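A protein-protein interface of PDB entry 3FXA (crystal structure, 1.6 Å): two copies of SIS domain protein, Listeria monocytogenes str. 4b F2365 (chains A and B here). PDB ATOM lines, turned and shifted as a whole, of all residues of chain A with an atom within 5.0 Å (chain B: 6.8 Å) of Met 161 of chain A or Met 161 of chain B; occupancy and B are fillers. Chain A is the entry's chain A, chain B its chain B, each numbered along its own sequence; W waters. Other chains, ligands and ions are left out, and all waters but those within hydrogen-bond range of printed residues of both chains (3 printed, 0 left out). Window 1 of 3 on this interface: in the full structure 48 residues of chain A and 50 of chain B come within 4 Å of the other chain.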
ATOM      1  N   GLU A  18      -6.706  -7.477  16.417  1.00  0.00           N
ATOM      2  CA  GLU A  18      -7.278  -7.853  17.730  1.00  0.00           C
ATOM      3  C   GLU A  18      -6.739  -6.958  18.847  1.00  0.00           C
ATOM      4  O   GLU A  18      -7.510  -6.468  19.665  1.00  0.00           O
ATOM      5  CB  GLU A  18      -7.070  -9.336  18.039  1.00  0.00           C
ATOM      6  CG  GLU A  18      -7.948 -10.185  17.130  1.00  0.00           C
ATOM      7  CD  GLU A  18      -7.995 -11.634  17.546  1.00  0.00           C
ATOM      8  OE1 GLU A  18      -6.979 -12.204  17.992  1.00  0.00           O
ATOM      9  OE2 GLU A  18      -9.084 -12.207  17.417  1.00  0.00           O
ATOM     10  N   ILE A  22      -9.047  -4.144  21.266  1.00  0.00           N
ATOM     11  CA  ILE A  22      -9.043  -4.045  22.732  1.00  0.00           C
ATOM     12  C   ILE A  22      -8.544  -2.667  23.138  1.00  0.00           C
ATOM     13  O   ILE A  22      -9.105  -2.062  24.044  1.00  0.00           O
ATOM     14  CB  ILE A  22      -8.142  -5.089  23.395  1.00  0.00           C
ATOM     15  CG1 ILE A  22      -8.613  -6.487  23.022  1.00  0.00           C
ATOM     16  CG2 ILE A  22      -8.128  -4.938  24.934  1.00  0.00           C
ATOM     17  CD1 ILE A  22      -7.731  -7.494  23.516  1.00  0.00           C
ATOM     18  N   THR A 157     -14.118 -12.457  15.378  1.00  0.00           N
ATOM     19  CA  THR A 157     -13.040 -12.778  16.334  1.00  0.00           C
ATOM     20  C   THR A 157     -12.710 -11.532  17.188  1.00  0.00           C
ATOM     21  O   THR A 157     -12.733 -11.585  18.420  1.00  0.00           O
ATOM     22  CB  THR A 157     -11.760 -13.292  15.611  1.00  0.00           C
ATOM     23  OG1 THR A 157     -11.389 -12.375  14.582  1.00  0.00           O
ATOM     24  CG2 THR A 157     -11.971 -14.684  14.980  1.00  0.00           C
ATOM     25  N   ALA A 158     -12.431 -10.414  16.535  1.00  0.00           N
ATOM     26  CA  ALA A 158     -12.195  -9.158  17.258  1.00  0.00           C
ATOM     27  C   ALA A 158     -13.409  -8.746  18.115  1.00  0.00           C
ATOM     28  O   ALA A 158     -13.240  -8.342  19.284  1.00  0.00           O
ATOM     29  CB  ALA A 158     -11.829  -8.036  16.297  1.00  0.00           C
ATOM     30  N   SER A 159     -14.624  -8.883  17.560  1.00  0.00           N
ATOM     31  CA  SER A 159     -15.864  -8.531  18.299  1.00  0.00           C
ATOM     32  C   SER A 159     -15.999  -9.348  19.582  1.00  0.00           C
ATOM     33  O   SER A 159     -16.338  -8.807  20.649  1.00  0.00           O
ATOM     34  CB  SER A 159     -17.110  -8.708  17.408  1.00  0.00           C
ATOM     35  OG  SER A 159     -18.315  -8.462  18.110  1.00  0.00           O
ATOM     36  N   THR A 160     -15.746 -10.658  19.467  1.00  0.00           N
ATOM     37  CA  THR A 160     -15.792 -11.568  20.610  1.00  0.00           C
ATOM     38  C   THR A 160     -14.777 -11.178  21.682  1.00  0.00           C
ATOM     39  O   THR A 160     -15.116 -11.103  22.873  1.00  0.00           O
ATOM     40  CB  THR A 160     -15.554 -13.011  20.161  1.00  0.00           C
ATOM     41  OG1 THR A 160     -16.474 -13.309  19.092  1.00  0.00           O
ATOM     42  CG2 THR A 160     -15.748 -13.976  21.319  1.00  0.00           C
ATOM     43  N   MET A 161     -13.554 -10.884  21.230  1.00  0.00           N
ATOM     44  CA  MET A 161     -12.463 -10.491  22.115  1.00  0.00           C
ATOM     45  C   MET A 161     -12.790  -9.179  22.830  1.00  0.00           C
ATOM     46  O   MET A 161     -12.548  -9.069  24.033  1.00  0.00           O
ATOM     47  CB  MET A 161     -11.143 -10.372  21.351  1.00  0.00           C
ATOM     48  CG  MET A 161      -9.964 -10.396  22.256  1.00  0.00           C
ATOM     49  SD  MET A 161      -8.398 -10.908  21.272  1.00  0.00           S
ATOM     50  CE  MET A 161      -8.944 -12.658  20.662  1.00  0.00           C
ATOM     51  N   ALA A 162     -13.365  -8.218  22.094  1.00  0.00           N
ATOM     52  CA  ALA A 162     -13.774  -6.920  22.658  1.00  0.00           C
ATOM     53  C   ALA A 162     -14.827  -7.112  23.773  1.00  0.00           C
ATOM     54  O   ALA A 162     -14.740  -6.506  24.848  1.00  0.00           O
ATOM     55  CB  ALA A 162     -14.316  -5.987  21.583  1.00  0.00           C
ATOM     56  N   VAL A 163     -15.799  -7.984  23.528  1.00  0.00           N
ATOM     57  CA  VAL A 163     -16.779  -8.328  24.572  1.00  0.00           C
ATOM     58  C   VAL A 163     -16.130  -8.990  25.802  1.00  0.00           C
ATOM     59  O   VAL A 163     -16.381  -8.555  26.915  1.00  0.00           O
ATOM     60  CB  VAL A 163     -17.954  -9.209  24.052  1.00  0.00           C
ATOM     61  CG1 VAL A 163     -18.888  -9.569  25.194  1.00  0.00           C
ATOM     62  CG2 VAL A 163     -18.728  -8.502  22.966  1.00  0.00           C
ATOM     63  N   ILE A 164     -15.266  -9.982  25.591  1.00  0.00           N
ATOM     64  CA  ILE A 164     -14.619 -10.680  26.700  1.00  0.00           C
ATOM     65  C   ILE A 164     -13.783  -9.665  27.505  1.00  0.00           C
ATOM     66  O   ILE A 164     -13.919  -9.587  28.730  1.00  0.00           O
ATOM     67  CB  ILE A 164     -13.742 -11.864  26.227  1.00  0.00           C
ATOM     68  CG1 ILE A 164     -14.621 -12.981  25.641  1.00  0.00           C
ATOM     69  CG2 ILE A 164     -12.930 -12.407  27.402  1.00  0.00           C
ATOM     70  CD1 ILE A 164     -13.813 -14.128  25.018  1.00  0.00           C
ATOM     71  N   ALA A 165     -12.933  -8.909  26.805  1.00  0.00           N
ATOM     72  CA  ALA A 165     -12.099  -7.878  27.445  1.00  0.00           C
ATOM     73  C   ALA A 165     -12.913  -6.857  28.228  1.00  0.00           C
ATOM     74  O   ALA A 165     -12.505  -6.444  29.333  1.00  0.00           O
ATOM     75  CB  ALA A 165     -11.256  -7.159  26.412  1.00  0.00           C
ATOM     76  N   SER A 166     -14.060  -6.434  27.674  1.00  0.00           N
ATOM     77  CA  SER A 166     -14.948  -5.498  28.376  1.00  0.00           C
ATOM     78  C   SER A 166     -15.348  -6.032  29.766  1.00  0.00           C
ATOM     79  O   SER A 166     -15.166  -5.373  30.768  1.00  0.00           O
ATOM     80  CB  SER A 166     -16.191  -5.177  27.557  1.00  0.00           C
ATOM     81  OG  SER A 166     -15.896  -4.502  26.358  1.00  0.00           O
ATOM     82  N   ASP A 168     -13.849  -8.628  31.349  1.00  0.00           N
ATOM     83  CA  ASP A 168     -12.631  -8.914  32.127  1.00  0.00           C
ATOM     84  C   ASP A 168     -12.329  -7.688  33.002  1.00  0.00           C
ATOM     85  O   ASP A 168     -12.035  -7.835  34.166  1.00  0.00           O
ATOM     86  CB  ASP A 168     -11.413  -9.240  31.220  1.00  0.00           C
ATOM     87  CG  ASP A 168     -11.458 -10.643  30.633  1.00  0.00           C
ATOM     88  OD1 ASP A 168     -12.167 -11.505  31.167  1.00  0.00           O
ATOM     89  OD2 ASP A 168     -10.745 -10.896  29.629  1.00  0.00           O
ATOM     90  N   GLU B  18      -4.326  -6.270  28.587  1.00  0.00           N
ATOM     91  CA  GLU B  18      -4.860  -7.250  27.628  1.00  0.00           C
ATOM     92  C   GLU B  18      -4.428  -6.945  26.192  1.00  0.00           C
ATOM     93  O   GLU B  18      -4.057  -7.848  25.450  1.00  0.00           O
ATOM     94  CB  GLU B  18      -6.381  -7.415  27.780  1.00  0.00           C
ATOM     95  CG  GLU B  18      -6.732  -8.141  29.040  1.00  0.00           C
ATOM     96  CD  GLU B  18      -8.191  -8.545  29.114  1.00  0.00           C
ATOM     97  OE1 GLU B  18      -9.070  -7.716  28.802  1.00  0.00           O
ATOM     98  OE2 GLU B  18      -8.432  -9.701  29.518  1.00  0.00           O
ATOM     99  N   ALA B  19      -4.451  -5.682  25.788  1.00  0.00           N
ATOM    100  CA  ALA B  19      -3.967  -5.309  24.444  1.00  0.00           C
ATOM    101  C   ALA B  19      -2.482  -5.628  24.317  1.00  0.00           C
ATOM    102  O   ALA B  19      -2.065  -6.130  23.279  1.00  0.00           O
ATOM    103  CB  ALA B  19      -4.203  -3.829  24.169  1.00  0.00           C
ATOM    104  N   ALA B  21      -0.804  -7.929  25.883  1.00  0.00           N
ATOM    105  CA  ALA B  21      -0.657  -9.399  25.804  1.00  0.00           C
ATOM    106  C   ALA B  21      -0.780  -9.924  24.376  1.00  0.00           C
ATOM    107  O   ALA B  21      -0.001 -10.778  23.938  1.00  0.00           O
ATOM    108  CB  ALA B  21      -1.719 -10.069  26.708  1.00  0.00           C
ATOM    109  N   ILE B  22      -1.734  -9.365  23.640  1.00  0.00           N
ATOM    110  CA  ILE B  22      -1.989  -9.757  22.257  1.00  0.00           C
ATOM    111  C   ILE B  22      -0.896  -9.196  21.342  1.00  0.00           C
ATOM    112  O   ILE B  22      -0.327  -9.927  20.512  1.00  0.00           O
ATOM    113  CB  ILE B  22      -3.359  -9.285  21.779  1.00  0.00           C
ATOM    114  CG1 ILE B  22      -4.440  -9.910  22.672  1.00  0.00           C
ATOM    115  CG2 ILE B  22      -3.591  -9.688  20.296  1.00  0.00           C
ATOM    116  CD1 ILE B  22      -5.747  -9.423  22.349  1.00  0.00           C
ATOM    117  N   LEU B  25       2.274 -11.155  21.262  1.00  0.00           N
ATOM    118  CA  LEU B  25       2.254 -12.583  20.855  1.00  0.00           C
ATOM    119  C   LEU B  25       3.463 -13.094  20.037  1.00  0.00           C
ATOM    120  O   LEU B  25       3.866 -14.210  20.271  1.00  0.00           O
ATOM    121  CB  LEU B  25       0.926 -12.966  20.172  1.00  0.00           C
ATOM    122  CG  LEU B  25      -0.239 -13.206  21.132  1.00  0.00           C
ATOM    123  CD1 LEU B  25      -1.539 -13.225  20.331  1.00  0.00           C
ATOM    124  CD2 LEU B  25      -0.021 -14.518  21.894  1.00  0.00           C
ATOM    125  N   THR B  55     -10.835 -21.527  32.980  1.00  0.00           N
ATOM    126  CA  THR B  55     -10.665 -20.500  31.938  1.00  0.00           C
ATOM    127  C   THR B  55     -10.005 -21.078  30.665  1.00  0.00           C
ATOM    128  O   THR B  55     -10.334 -20.630  29.566  1.00  0.00           O
ATOM    129  CB  THR B  55      -9.985 -19.217  32.485  1.00  0.00           C
ATOM    130  OG1 THR B  55     -10.123 -18.145  31.554  1.00  0.00           O
ATOM    131  CG2 THR B  55      -8.539 -19.467  32.842  1.00  0.00           C
ATOM    132  N   ALA B  59     -11.388 -21.001  26.744  1.00  0.00           N
ATOM    133  CA  ALA B  59     -10.539 -20.809  25.568  1.00  0.00           C
ATOM    134  C   ALA B  59     -10.732 -22.031  24.639  1.00  0.00           C
ATOM    135  O   ALA B  59     -10.959 -21.896  23.424  1.00  0.00           O
ATOM    136  CB  ALA B  59      -9.074 -20.653  25.962  1.00  0.00           C
ATOM    137  N   LYS B  62     -13.780 -21.817  22.623  1.00  0.00           N
ATOM    138  CA  LYS B  62     -13.652 -20.789  21.611  1.00  0.00           C
ATOM    139  C   LYS B  62     -12.980 -21.429  20.378  1.00  0.00           C
ATOM    140  O   LYS B  62     -13.481 -21.274  19.271  1.00  0.00           O
ATOM    141  CB  LYS B  62     -12.866 -19.569  22.135  1.00  0.00           C
ATOM    142  CG  LYS B  62     -13.266 -18.251  21.467  1.00  0.00           C
ATOM    143  CD  LYS B  62     -12.874 -18.082  20.033  1.00  0.00           C
ATOM    144  CE  LYS B  62     -13.489 -16.871  19.367  1.00  0.00           C
ATOM    145  NZ  LYS B  62     -13.001 -16.731  17.960  1.00  0.00           N
ATOM    146  N   VAL B 143       2.725 -20.356  24.442  1.00  0.00           N
ATOM    147  CA  VAL B 143       1.954 -19.120  24.597  1.00  0.00           C
ATOM    148  C   VAL B 143       2.051 -18.716  26.060  1.00  0.00           C
ATOM    149  O   VAL B 143       1.968 -19.563  26.963  1.00  0.00           O
ATOM    150  CB  VAL B 143       0.454 -19.226  24.130  1.00  0.00           C
ATOM    151  CG1 VAL B 143      -0.263 -20.331  24.860  1.00  0.00           C
ATOM    152  CG2 VAL B 143      -0.301 -17.868  24.293  1.00  0.00           C
ATOM    153  N   VAL B 145       2.020 -14.831  28.827  1.00  0.00           N
ATOM    154  CA  VAL B 145       1.919 -13.374  29.079  1.00  0.00           C
ATOM    155  C   VAL B 145       2.820 -13.000  30.257  1.00  0.00           C
ATOM    156  O   VAL B 145       2.990 -13.788  31.211  1.00  0.00           O
ATOM    157  CB  VAL B 145       0.442 -12.893  29.311  1.00  0.00           C
ATOM    158  CG1 VAL B 145      -0.467 -13.261  28.118  1.00  0.00           C
ATOM    159  CG2 VAL B 145      -0.151 -13.422  30.603  1.00  0.00           C
ATOM    160  N   ALA B 156      -5.859 -15.218  35.319  1.00  0.00           N
ATOM    161  CA  ALA B 156      -5.425 -15.657  33.969  1.00  0.00           C
ATOM    162  C   ALA B 156      -6.241 -15.060  32.797  1.00  0.00           C
ATOM    163  O   ALA B 156      -6.386 -15.686  31.754  1.00  0.00           O
ATOM    164  CB  ALA B 156      -5.357 -17.170  33.882  1.00  0.00           C
ATOM    165  N   THR B 157      -6.694 -13.814  32.947  1.00  0.00           N
ATOM    166  CA  THR B 157      -7.495 -13.131  31.929  1.00  0.00           C
ATOM    167  C   THR B 157      -6.670 -12.849  30.670  1.00  0.00           C
ATOM    168  O   THR B 157      -7.098 -13.182  29.565  1.00  0.00           O
ATOM    169  CB  THR B 157      -8.175 -11.818  32.462  1.00  0.00           C
ATOM    170  OG1 THR B 157      -7.182 -10.843  32.795  1.00  0.00           O
ATOM    171  CG2 THR B 157      -9.030 -12.090  33.693  1.00  0.00           C
ATOM    172  N   ALA B 158      -5.483 -12.251  30.833  1.00  0.00           N
ATOM    173  CA  ALA B 158      -4.611 -11.997  29.663  1.00  0.00           C
ATOM    174  C   ALA B 158      -4.109 -13.293  29.007  1.00  0.00           C
ATOM    175  O   ALA B 158      -4.039 -13.365  27.784  1.00  0.00           O
ATOM    176  CB  ALA B 158      -3.460 -11.095  30.016  1.00  0.00           C
ATOM    177  N   SER B 159      -3.757 -14.283  29.835  1.00  0.00           N
ATOM    178  CA  SER B 159      -3.336 -15.647  29.426  1.00  0.00           C
ATOM    179  C   SER B 159      -4.404 -16.257  28.542  1.00  0.00           C
ATOM    180  O   SER B 159      -4.121 -16.718  27.439  1.00  0.00           O
ATOM    181  CB  SER B 159      -3.114 -16.541  30.662  1.00  0.00           C
ATOM    182  OG  SER B 159      -2.854 -17.895  30.338  1.00  0.00           O
ATOM    183  N   THR B 160      -5.638 -16.198  29.032  1.00  0.00           N
ATOM    184  CA  THR B 160      -6.797 -16.747  28.277  1.00  0.00           C
ATOM    185  C   THR B 160      -6.970 -16.081  26.943  1.00  0.00           C
ATOM    186  O   THR B 160      -7.132 -16.752  25.927  1.00  0.00           O
ATOM    187  CB  THR B 160      -8.065 -16.650  29.086  1.00  0.00           C
ATOM    188  OG1 THR B 160      -7.882 -17.464  30.236  1.00  0.00           O
ATOM    189  CG2 THR B 160      -9.312 -17.219  28.290  1.00  0.00           C
ATOM    190  N   MET B 161      -6.903 -14.758  26.958  1.00  0.00           N
ATOM    191  CA  MET B 161      -7.009 -13.937  25.767  1.00  0.00           C
ATOM    192  C   MET B 161      -5.875 -14.198  24.766  1.00  0.00           C
ATOM    193  O   MET B 161      -6.101 -14.203  23.568  1.00  0.00           O
ATOM    194  CB  MET B 161      -7.047 -12.475  26.170  1.00  0.00           C
ATOM    195  CG  MET B 161      -7.242 -11.552  25.020  1.00  0.00           C
ATOM    196  SD  MET B 161      -8.238 -10.021  25.563  1.00  0.00           S
ATOM    197  CE  MET B 161      -9.879 -11.028  25.840  1.00  0.00           C
ATOM    198  N   ALA B 162      -4.677 -14.427  25.286  1.00  0.00           N
ATOM    199  CA  ALA B 162      -3.492 -14.705  24.433  1.00  0.00           C
ATOM    200  C   ALA B 162      -3.678 -16.055  23.683  1.00  0.00           C
ATOM    201  O   ALA B 162      -3.332 -16.158  22.496  1.00  0.00           O
ATOM    202  CB  ALA B 162      -2.220 -14.704  25.249  1.00  0.00           C
ATOM    203  N   VAL B 163      -4.233 -17.067  24.357  1.00  0.00           N
ATOM    204  CA  VAL B 163      -4.494 -18.376  23.714  1.00  0.00           C
ATOM    205  C   VAL B 163      -5.564 -18.240  22.634  1.00  0.00           C
ATOM    206  O   VAL B 163      -5.397 -18.754  21.523  1.00  0.00           O
ATOM    207  CB  VAL B 163      -4.878 -19.492  24.737  1.00  0.00           C
ATOM    208  CG1 VAL B 163      -5.354 -20.799  24.012  1.00  0.00           C
ATOM    209  CG2 VAL B 163      -3.727 -19.743  25.685  1.00  0.00           C
ATOM    210  N   ILE B 164      -6.656 -17.537  22.950  1.00  0.00           N
ATOM    211  CA  ILE B 164      -7.775 -17.344  22.017  1.00  0.00           C
ATOM    212  C   ILE B 164      -7.264 -16.623  20.785  1.00  0.00           C
ATOM    213  O   ILE B 164      -7.475 -17.125  19.666  1.00  0.00           O
ATOM    214  CB  ILE B 164      -8.996 -16.613  22.661  1.00  0.00           C
ATOM    215  CG1 ILE B 164      -9.656 -17.486  23.730  1.00  0.00           C
ATOM    216  CG2 ILE B 164     -10.010 -16.167  21.575  1.00  0.00           C
ATOM    217  CD1 ILE B 164     -10.788 -16.762  24.488  1.00  0.00           C
ATOM    218  N   ALA B 165      -6.527 -15.522  20.999  1.00  0.00           N
ATOM    219  CA  ALA B 165      -5.922 -14.745  19.895  1.00  0.00           C
ATOM    220  C   ALA B 165      -4.995 -15.586  19.032  1.00  0.00           C
ATOM    221  O   ALA B 165      -5.022 -15.481  17.787  1.00  0.00           O
ATOM    222  CB  ALA B 165      -5.135 -13.561  20.411  1.00  0.00           C
ATOM    223  N   SER B 166      -4.160 -16.400  19.671  1.00  0.00           N
ATOM    224  CA  SER B 166      -3.237 -17.294  18.947  1.00  0.00           C
ATOM    225  C   SER B 166      -3.995 -18.172  17.950  1.00  0.00           C
ATOM    226  O   SER B 166      -3.682 -18.208  16.755  1.00  0.00           O
ATOM    227  CB  SER B 166      -2.421 -18.165  19.893  1.00  0.00           C
ATOM    228  OG  SER B 166      -1.607 -17.392  20.773  1.00  0.00           O
ATOM    229  N   ASP B 168      -7.196 -17.730  16.989  1.00  0.00           N
ATOM    230  CA  ASP B 168      -7.927 -16.865  16.053  1.00  0.00           C
ATOM    231  C   ASP B 168      -7.069 -16.643  14.812  1.00  0.00           C
ATOM    232  O   ASP B 168      -7.566 -16.844  13.711  1.00  0.00           O
ATOM    233  CB  ASP B 168      -8.340 -15.517  16.651  1.00  0.00           C
ATOM    234  CG  ASP B 168      -9.526 -15.624  17.629  1.00  0.00           C
ATOM    235  OD1 ASP B 168     -10.217 -16.673  17.681  1.00  0.00           O
ATOM    236  OD2 ASP B 168      -9.796 -14.619  18.285  1.00  0.00           O
HETATM  237  O   HOH W   1     -12.011 -14.001  19.466  1.00  0.00           O
HETATM  238  O   HOH W   2      -9.857 -13.378  29.169  1.00  0.00           O
HETATM  239  O   HOH W   3     -15.170 -15.287  16.644  1.00  0.00           O
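OE2 of Glu 18 of chain A lies close to OD2 of Asp 168 of chain B.
OD2 of Asp 168 of chain A sits close to OE2 of Glu 18 of chain B, at 2.6 Å.
Of the 22 printed residues of chain B, 9 touch a printed residue of chain A.
Printed residues of chain B that touch a printed residue of chain A: Glu 18, Ala 19, Ile 22, Lys 62, Thr 157, Met 161, Ile 164, Ala 165 and Asp 168.
Hydrophobic or aromatic side chains of chain B that line the printed part of chain A: Ile 22, Met 161, Ile 164 and Ala 165.
Of the 13 printed residues of chain A, 7 touch a printed residue of chain B.
Printed residues of chain B within 4 Å of Ile 22 of chain A: Ala 19, Ile 22 and Met 161.
Of the printed residues of chain B, Met 161 of chain A touches Ile 22 (3.2 Å), Met 161 (3.6 Å), Ile 164 (3.8 Å), Ala 165 (3.8 Å) and Asp 168 (3.2 Å).
Of the printed residues of chain B, Ile 164 of chain A touches Met 161.
Printed residues of chain A within 4 Å of Ile 22 of chain B: Ile 22 (3.0 Å) and Met 161 (3.2 Å).
Ser 159 of chain B touches none of the printed residues of chain A.
Of the printed residues of chain A, Met 161 of chain B touches Ile 22 (3.3 Å), Met 161 (3.6 Å), Ile 164 (3.7 Å), Ala 165 (3.8 Å) and Asp 168 (3.9 Å).
The nearest printed residue of chain B that does not touch Met 161 of chain A is Glu 18 of chain B (6.1 Å).
The side-chain carboxylate of Asp 168 of chain B lies within salt-bridge range of the side-chain amino group of Lys 62 of chain B, 2.8 Å away.
Glu 18 of chain A touches Asp 168 of chain B, and with the chains exchanged Asp 168 of chain A touches Glu 18 of chain B.
Ile 22 of chain A touches its own counterpart, Ile 22 of chain B.
Thr 157 of chain A touches Asp 168 of chain B, and with the chains exchanged Asp 168 of chain A touches Thr 157 of chain B.
Met 161 of chain A touches Ala 165 of chain B, and with the chains exchanged Ala 165 of chain A touches Met 161 of chain B.
13 positions are printed for both chains.
Among the printed residues, merely in contact across the chains: Ile 22 of chain A with Ile 22 of chain B (3.0 Å), Met 161 of chain A with Asp 168 of chain B (3.2 Å), Met 161 of chain A with Ile 22 of chain B (3.2 Å), Ala 165 of chain A with Glu 18 of chain B (3.3 Å), Ile 22 of chain A with Met 161 of chain B (3.3 Å), Glu 18 of chain A with Ala 165 of chain B (3.3 Å), Thr 157 of chain A with Asp 168 of chain B (3.6 Å), Met 161 of chain A with Met 161 of chain B (3.6 Å), Ile 164 of chain A with Met 161 of chain B (3.7 Å), Met 161 of chain A with Ala 165 of chain B (3.8 Å), Thr 157 of chain A with Lys 62 of chain B (3.8 Å), Met 161 of chain A with Ile 164 of chain B (3.8 Å), Ala 165 of chain A with Met 161 of chain B (3.8 Å), Ile 22 of chain A with Ala 19 of chain B (3.8 Å), Asp 168 of chain A with Met 161 of chain B (3.9 Å) and Asp 168 of chain A with Thr 157 of chain B (3.9 Å).
Water W1 lies within hydrogen-bond range of OD2 of Asp 168 of chain B (2.6 Å), O of Thr 157 of chain A (2.7 Å) and NZ of Lys 62 of chain B (3.3 Å).
Water W2 lies within hydrogen-bond range of OD2 of Asp 168 of chain A (2.7 Å) and O of Thr 157 of chain B (2.8 Å).
Water W3 lies within hydrogen-bond range of NZ of Lys 62 of chain B, N of Thr 157 of chain A and OG1 of Thr 160 of chain A.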
